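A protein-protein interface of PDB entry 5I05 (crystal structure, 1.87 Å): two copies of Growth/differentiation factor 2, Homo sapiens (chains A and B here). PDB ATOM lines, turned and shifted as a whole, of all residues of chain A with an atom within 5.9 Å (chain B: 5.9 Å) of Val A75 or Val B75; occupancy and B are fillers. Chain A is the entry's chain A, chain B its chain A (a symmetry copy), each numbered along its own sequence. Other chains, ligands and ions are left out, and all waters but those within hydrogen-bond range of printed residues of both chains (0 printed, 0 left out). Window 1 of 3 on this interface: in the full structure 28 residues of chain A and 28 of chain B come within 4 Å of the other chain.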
ATOM      1  N   CYS A   8      17.214  29.377   0.700  1.00  0.00           N
ATOM      2  CA  CYS A   8      15.791  29.691   0.716  1.00  0.00           C
ATOM      3  C   CYS A   8      15.202  29.442   2.098  1.00  0.00           C
ATOM      4  O   CYS A   8      15.226  28.315   2.600  1.00  0.00           O
ATOM      5  CB  CYS A   8      15.082  28.838  -0.337  1.00  0.00           C
ATOM      6  SG  CYS A   8      13.319  29.104  -0.498  1.00  0.00           S
ATOM      7  N   CYS A  37       9.492  34.511   1.636  1.00  0.00           N
ATOM      8  CA  CYS A  37      10.537  33.534   1.337  1.00  0.00           C
ATOM      9  C   CYS A  37      11.681  34.235   0.622  1.00  0.00           C
ATOM     10  O   CYS A  37      11.486  34.796  -0.463  1.00  0.00           O
ATOM     11  CB  CYS A  37       9.977  32.387   0.494  1.00  0.00           C
ATOM     12  SG  CYS A  37       8.681  31.475   1.354  1.00  0.00           S
ATOM     13  N   CYS A  73      13.318  29.474  -8.145  1.00  0.00           N
ATOM     14  CA  CYS A  73      12.885  30.605  -7.333  1.00  0.00           C
ATOM     15  C   CYS A  73      12.453  30.138  -5.952  1.00  0.00           C
ATOM     16  O   CYS A  73      11.770  29.120  -5.812  1.00  0.00           O
ATOM     17  CB  CYS A  73      11.740  31.363  -8.021  1.00  0.00           C
ATOM     18  SG  CYS A  73      12.155  32.025  -9.667  1.00  0.00           S
ATOM     19  N   CYS A  74      12.854  30.893  -4.934  1.00  0.00           N
ATOM     20  CA  CYS A  74      12.476  30.619  -3.554  1.00  0.00           C
ATOM     21  C   CYS A  74      11.087  31.201  -3.303  1.00  0.00           C
ATOM     22  O   CYS A  74      10.919  32.423  -3.351  1.00  0.00           O
ATOM     23  CB  CYS A  74      13.514  31.239  -2.614  1.00  0.00           C
ATOM     24  SG  CYS A  74      13.177  31.086  -0.884  1.00  0.00           S
ATOM     25  N   VAL A  75      10.103  30.338  -3.045  1.00  0.00           N
ATOM     26  CA  VAL A  75       8.702  30.759  -2.949  1.00  0.00           C
ATOM     27  C   VAL A  75       8.021  30.045  -1.792  1.00  0.00           C
ATOM     28  O   VAL A  75       8.496  29.014  -1.300  1.00  0.00           O
ATOM     29  CB  VAL A  75       7.923  30.477  -4.252  1.00  0.00           C
ATOM     30  CG1 VAL A  75       8.382  31.411  -5.360  1.00  0.00           C
ATOM     31  CG2 VAL A  75       8.096  29.023  -4.653  1.00  0.00           C
ATOM     32  N   PRO A  76       6.885  30.577  -1.339  1.00  0.00           N
ATOM     33  CA  PRO A  76       6.067  29.829  -0.382  1.00  0.00           C
ATOM     34  C   PRO A  76       5.543  28.555  -1.026  1.00  0.00           C
ATOM     35  O   PRO A  76       5.040  28.564  -2.155  1.00  0.00           O
ATOM     36  CB  PRO A  76       4.940  30.809  -0.019  1.00  0.00           C
ATOM     37  CG  PRO A  76       5.454  32.148  -0.405  1.00  0.00           C
ATOM     38  CD  PRO A  76       6.355  31.929  -1.579  1.00  0.00           C
ATOM     39  N   THR A  77       5.702  27.450  -0.308  1.00  0.00           N
ATOM     40  CA  THR A  77       5.201  26.151  -0.727  1.00  0.00           C
ATOM     41  C   THR A  77       4.038  25.678   0.128  1.00  0.00           C
ATOM     42  O   THR A  77       3.377  24.700  -0.235  1.00  0.00           O
ATOM     43  CB  THR A  77       6.332  25.111  -0.676  1.00  0.00           C
ATOM     44  OG1 THR A  77       6.905  25.099   0.634  1.00  0.00           O
ATOM     45  CG2 THR A  77       7.414  25.455  -1.696  1.00  0.00           C
ATOM     46  N   GLU A 106       5.689  27.459   4.925  1.00  0.00           N
ATOM     47  CA  GLU A 106       6.936  26.836   4.501  1.00  0.00           C
ATOM     48  C   GLU A 106       7.389  27.439   3.181  1.00  0.00           C
ATOM     49  O   GLU A 106       6.568  27.840   2.358  1.00  0.00           O
ATOM     50  CB  GLU A 106       6.779  25.323   4.347  1.00  0.00           C
ATOM     51  CG  GLU A 106       6.361  24.629   5.624  1.00  0.00           C
ATOM     52  CD  GLU A 106       6.470  23.132   5.530  1.00  0.00           C
ATOM     53  OE1 GLU A 106       6.710  22.498   6.577  1.00  0.00           O
ATOM     54  OE2 GLU A 106       6.326  22.598   4.411  1.00  0.00           O
ATOM     55  N   CYS A 107       8.709  27.472   2.988  1.00  0.00           N
ATOM     56  CA  CYS A 107       9.360  27.978   1.788  1.00  0.00           C
ATOM     57  C   CYS A 107      10.101  26.836   1.104  1.00  0.00           C
ATOM     58  O   CYS A 107      10.501  25.861   1.748  1.00  0.00           O
ATOM     59  CB  CYS A 107      10.367  29.097   2.113  1.00  0.00           C
ATOM     60  SG  CYS A 107       9.692  30.585   2.872  1.00  0.00           S
ATOM     61  N   GLY A 108      10.297  26.975  -0.205  1.00  0.00           N
ATOM     62  CA  GLY A 108      11.093  26.010  -0.949  1.00  0.00           C
ATOM     63  C   GLY A 108      11.442  26.547  -2.319  1.00  0.00           C
ATOM     64  O   GLY A 108      10.895  27.549  -2.782  1.00  0.00           O
ATOM     65  N   CYS A 109      12.369  25.853  -2.969  1.00  0.00           N
ATOM     66  CA  CYS A 109      12.784  26.188  -4.324  1.00  0.00           C
ATOM     67  C   CYS A 109      11.888  25.465  -5.326  1.00  0.00           C
ATOM     68  O   CYS A 109      11.686  24.248  -5.224  1.00  0.00           O
ATOM     69  CB  CYS A 109      14.260  25.814  -4.514  1.00  0.00           C
ATOM     70  SG  CYS A 109      15.387  26.891  -3.577  1.00  0.00           S
ATOM     71  N   ARG A 110      11.344  26.217  -6.284  1.00  0.00           N
ATOM     72  CA  ARG A 110      10.427  25.665  -7.287  1.00  0.00           C
ATOM     73  C   ARG A 110      10.772  26.142  -8.699  1.00  0.00           C
ATOM     74  O   ARG A 110      10.469  25.452  -9.677  1.00  0.00           O
ATOM     75  CB  ARG A 110       8.970  26.026  -6.941  1.00  0.00           C
ATOM     76  CG  ARG A 110       8.448  25.388  -5.645  1.00  0.00           C
ATOM     77  CD  ARG A 110       8.399  23.864  -5.750  1.00  0.00           C
ATOM     78  NE  ARG A 110       7.863  23.212  -4.557  1.00  0.00           N
ATOM     79  CZ  ARG A 110       8.594  22.772  -3.532  1.00  0.00           C
ATOM     80  NH1 ARG A 110       9.915  22.939  -3.504  1.00  0.00           N
ATOM     81  NH2 ARG A 110       7.995  22.182  -2.509  1.00  0.00           N
ATOM     82  OXT ARG A 110      11.365  27.207  -8.920  1.00  0.00           O
ATOM     83  N   CYS B   8       3.105  35.598 -16.469  1.00  0.00           N
ATOM     84  CA  CYS B   8       3.625  34.286 -16.105  1.00  0.00           C
ATOM     85  C   CYS B   8       3.009  33.203 -16.979  1.00  0.00           C
ATOM     86  O   CYS B   8       1.790  33.009 -16.978  1.00  0.00           O
ATOM     87  CB  CYS B   8       3.328  34.026 -14.628  1.00  0.00           C
ATOM     88  SG  CYS B   8       3.923  32.469 -13.975  1.00  0.00           S
ATOM     89  N   CYS B  37       8.793  28.215 -16.548  1.00  0.00           N
ATOM     90  CA  CYS B  37       7.824  29.276 -16.281  1.00  0.00           C
ATOM     91  C   CYS B  37       8.531  30.621 -16.345  1.00  0.00           C
ATOM     92  O   CYS B  37       9.461  30.872 -15.571  1.00  0.00           O
ATOM     93  CB  CYS B  37       7.156  29.066 -14.921  1.00  0.00           C
ATOM     94  SG  CYS B  37       6.230  27.520 -14.845  1.00  0.00           S
ATOM     95  N   CYS B  73       6.948  35.442  -7.602  1.00  0.00           N
ATOM     96  CA  CYS B  73       7.778  34.750  -8.581  1.00  0.00           C
ATOM     97  C   CYS B  73       6.934  33.806  -9.424  1.00  0.00           C
ATOM     98  O   CYS B  73       6.060  33.104  -8.909  1.00  0.00           O
ATOM     99  CB  CYS B  73       8.908  33.976  -7.886  1.00  0.00           C
ATOM    100  SG  CYS B  73      10.027  35.009  -6.886  1.00  0.00           S
ATOM    101  N   CYS B  74       7.206  33.795 -10.726  1.00  0.00           N
ATOM    102  CA  CYS B  74       6.532  32.907 -11.663  1.00  0.00           C
ATOM    103  C   CYS B  74       7.211  31.540 -11.615  1.00  0.00           C
ATOM    104  O   CYS B  74       8.382  31.427 -11.989  1.00  0.00           O
ATOM    105  CB  CYS B  74       6.600  33.510 -13.069  1.00  0.00           C
ATOM    106  SG  CYS B  74       5.908  32.525 -14.365  1.00  0.00           S
ATOM    107  N   VAL B  75       6.489  30.517 -11.155  1.00  0.00           N
ATOM    108  CA  VAL B  75       7.077  29.197 -10.908  1.00  0.00           C
ATOM    109  C   VAL B  75       6.126  28.106 -11.378  1.00  0.00           C
ATOM    110  O   VAL B  75       4.924  28.334 -11.563  1.00  0.00           O
ATOM    111  CB  VAL B  75       7.404  28.979  -9.414  1.00  0.00           C
ATOM    112  CG1 VAL B  75       8.577  29.850  -8.993  1.00  0.00           C
ATOM    113  CG2 VAL B  75       6.176  29.268  -8.569  1.00  0.00           C
ATOM    114  N   PRO B  76       6.646  26.894 -11.571  1.00  0.00           N
ATOM    115  CA  PRO B  76       5.757  25.755 -11.809  1.00  0.00           C
ATOM    116  C   PRO B  76       4.897  25.499 -10.582  1.00  0.00           C
ATOM    117  O   PRO B  76       5.385  25.474  -9.447  1.00  0.00           O
ATOM    118  CB  PRO B  76       6.721  24.594 -12.103  1.00  0.00           C
ATOM    119  CG  PRO B  76       8.005  25.243 -12.474  1.00  0.00           C
ATOM    120  CD  PRO B  76       8.065  26.524 -11.705  1.00  0.00           C
ATOM    121  N   THR B  77       3.600  25.345 -10.820  1.00  0.00           N
ATOM    122  CA  THR B  77       2.634  25.022  -9.784  1.00  0.00           C
ATOM    123  C   THR B  77       2.092  23.610  -9.921  1.00  0.00           C
ATOM    124  O   THR B  77       1.428  23.124  -8.999  1.00  0.00           O
ATOM    125  CB  THR B  77       1.470  26.025  -9.820  1.00  0.00           C
ATOM    126  OG1 THR B  77       0.903  26.045 -11.133  1.00  0.00           O
ATOM    127  CG2 THR B  77       1.964  27.424  -9.465  1.00  0.00           C
ATOM    128  N   GLU B 106       1.774  23.303 -15.279  1.00  0.00           N
ATOM    129  CA  GLU B 106       1.141  24.604 -15.114  1.00  0.00           C
ATOM    130  C   GLU B 106       2.085  25.546 -14.382  1.00  0.00           C
ATOM    131  O   GLU B 106       2.880  25.116 -13.547  1.00  0.00           O
ATOM    132  CB  GLU B 106      -0.173  24.492 -14.340  1.00  0.00           C
ATOM    133  CG  GLU B 106      -1.192  23.598 -15.012  1.00  0.00           C
ATOM    134  CD  GLU B 106      -2.557  23.708 -14.389  1.00  0.00           C
ATOM    135  OE1 GLU B 106      -3.548  23.510 -15.119  1.00  0.00           O
ATOM    136  OE2 GLU B 106      -2.631  23.998 -13.177  1.00  0.00           O
ATOM    137  N   CYS B 107       1.963  26.838 -14.693  1.00  0.00           N
ATOM    138  CA  CYS B 107       2.742  27.913 -14.096  1.00  0.00           C
ATOM    139  C   CYS B 107       1.806  28.839 -13.330  1.00  0.00           C
ATOM    140  O   CYS B 107       0.616  28.940 -13.641  1.00  0.00           O
ATOM    141  CB  CYS B 107       3.491  28.735 -15.161  1.00  0.00           C
ATOM    142  SG  CYS B 107       4.708  27.846 -16.148  1.00  0.00           S
ATOM    143  N   GLY B 108       2.361  29.531 -12.337  1.00  0.00           N
ATOM    144  CA  GLY B 108       1.601  30.535 -11.608  1.00  0.00           C
ATOM    145  C   GLY B 108       2.518  31.398 -10.771  1.00  0.00           C
ATOM    146  O   GLY B 108       3.695  31.092 -10.574  1.00  0.00           O
ATOM    147  N   CYS B 109       1.952  32.492 -10.274  1.00  0.00           N
ATOM    148  CA  CYS B 109       2.668  33.407  -9.396  1.00  0.00           C
ATOM    149  C   CYS B 109       2.503  32.956  -7.946  1.00  0.00           C
ATOM    150  O   CYS B 109       1.378  32.709  -7.490  1.00  0.00           O
ATOM    151  CB  CYS B 109       2.144  34.833  -9.606  1.00  0.00           C
ATOM    152  SG  CYS B 109       2.620  35.528 -11.219  1.00  0.00           S
ATOM    153  N   ARG B 110       3.622  32.842  -7.231  1.00  0.00           N
ATOM    154  CA  ARG B 110       3.619  32.375  -5.839  1.00  0.00           C
ATOM    155  C   ARG B 110       4.497  33.250  -4.943  1.00  0.00           C
ATOM    156  O   ARG B 110       4.255  33.337  -3.735  1.00  0.00           O
ATOM    157  CB  ARG B 110       4.072  30.904  -5.763  1.00  0.00           C
ATOM    158  CG  ARG B 110       3.117  29.909  -6.437  1.00  0.00           C
ATOM    159  CD  ARG B 110       1.758  29.876  -5.739  1.00  0.00           C
ATOM    160  NE  ARG B 110       0.827  28.907  -6.314  1.00  0.00           N
ATOM    161  CZ  ARG B 110      -0.060  29.175  -7.273  1.00  0.00           C
ATOM    162  NH1 ARG B 110      -0.136  30.384  -7.826  1.00  0.00           N
ATOM    163  NH2 ARG B 110      -0.863  28.215  -7.705  1.00  0.00           N
ATOM    164  OXT ARG B 110       5.456  33.901  -5.376  1.00  0.00           O
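Of the 12 printed residues of chain A, 4 touch a printed residue of chain B.
Hydrophobic or aromatic side chains of chain A that line the printed part of chain B: Val A75 and Pro A76.
Hydrophobic or aromatic side chains of chain B that line the printed part of chain A: Val B75 and Pro B76.
Among the printed residues, no Asp or Glu carboxylate lies within 4 Å of a Lys or Arg side-chain nitrogen of the other chain.
The backbone carbonyl oxygen of Cys A73 sits at hydrogen-bond distance from the backbone NH of Arg A110 (3.0 Å).
The backbone NH (N) of Arg B110 is in hydrogen-bond range of the backbone carbonyl oxygen (O) of Cys B73.
N of Val B75 lies within hydrogen-bond range of O of Gly B108, 2.9 Å away.
SG of Cys A74 forms a disulfide with SG of Cys A8 (2.0 Å).
SG of Cys A37 is disulfide-bonded to SG of Cys A107 (2.0 Å).
SG of Cys B74 is disulfide-bonded to SG of Cys B8 (2.0 Å).
Printed residues of chain B within 4 Å of Val A75: Cys B73 (3.6 Å), Val B75 (3.96 Å) and Arg B110 (3.8 Å).
Of the printed residues of chain A, Val B75 touches Cys A73 (3.6 Å), Val A75 (3.96 Å) and Arg A110 (3.8 Å).
Printed residues of chain A within 4 Å of Arg B110: Val A75 and Pro A76.
Printed residues of chain B within 4 Å of Pro A76: Arg B110.
Printed residues of chain B within 4 Å of Arg A110: Val B75 (3.8 Å) and Pro B76 (3.3 Å).
The nearest printed residue of chain A that does not touch Val B75 is Cys A74 (6.0 Å).
Cys B73 touches Cys A73 (CB to CB, 3.9 Å).
Cys A73 touches Val B75 (CB to CG1, 3.6 Å).
Val A75 touches Cys B73.
Val A75 touches Val B75 (CG1 to CG1, 3.96 Å).
CG1 of Val A75 touches OXT of Arg B110, at 3.8 Å.
O of Arg B110 touches CD of Pro A76 (3.3 Å).
Arg A110 touches Val B75.
CD of Pro B76 touches O of Arg A110, at 3.3 Å.
Cys A73 touches its own counterpart, Cys B73.
Cys A73 touches Val B75, and with the chains exchanged Val A75 touches Cys B73.
Val A75 touches its own counterpart, Val B75.
Val A75 touches Arg B110, and with the chains exchanged Arg A110 touches Val B75.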
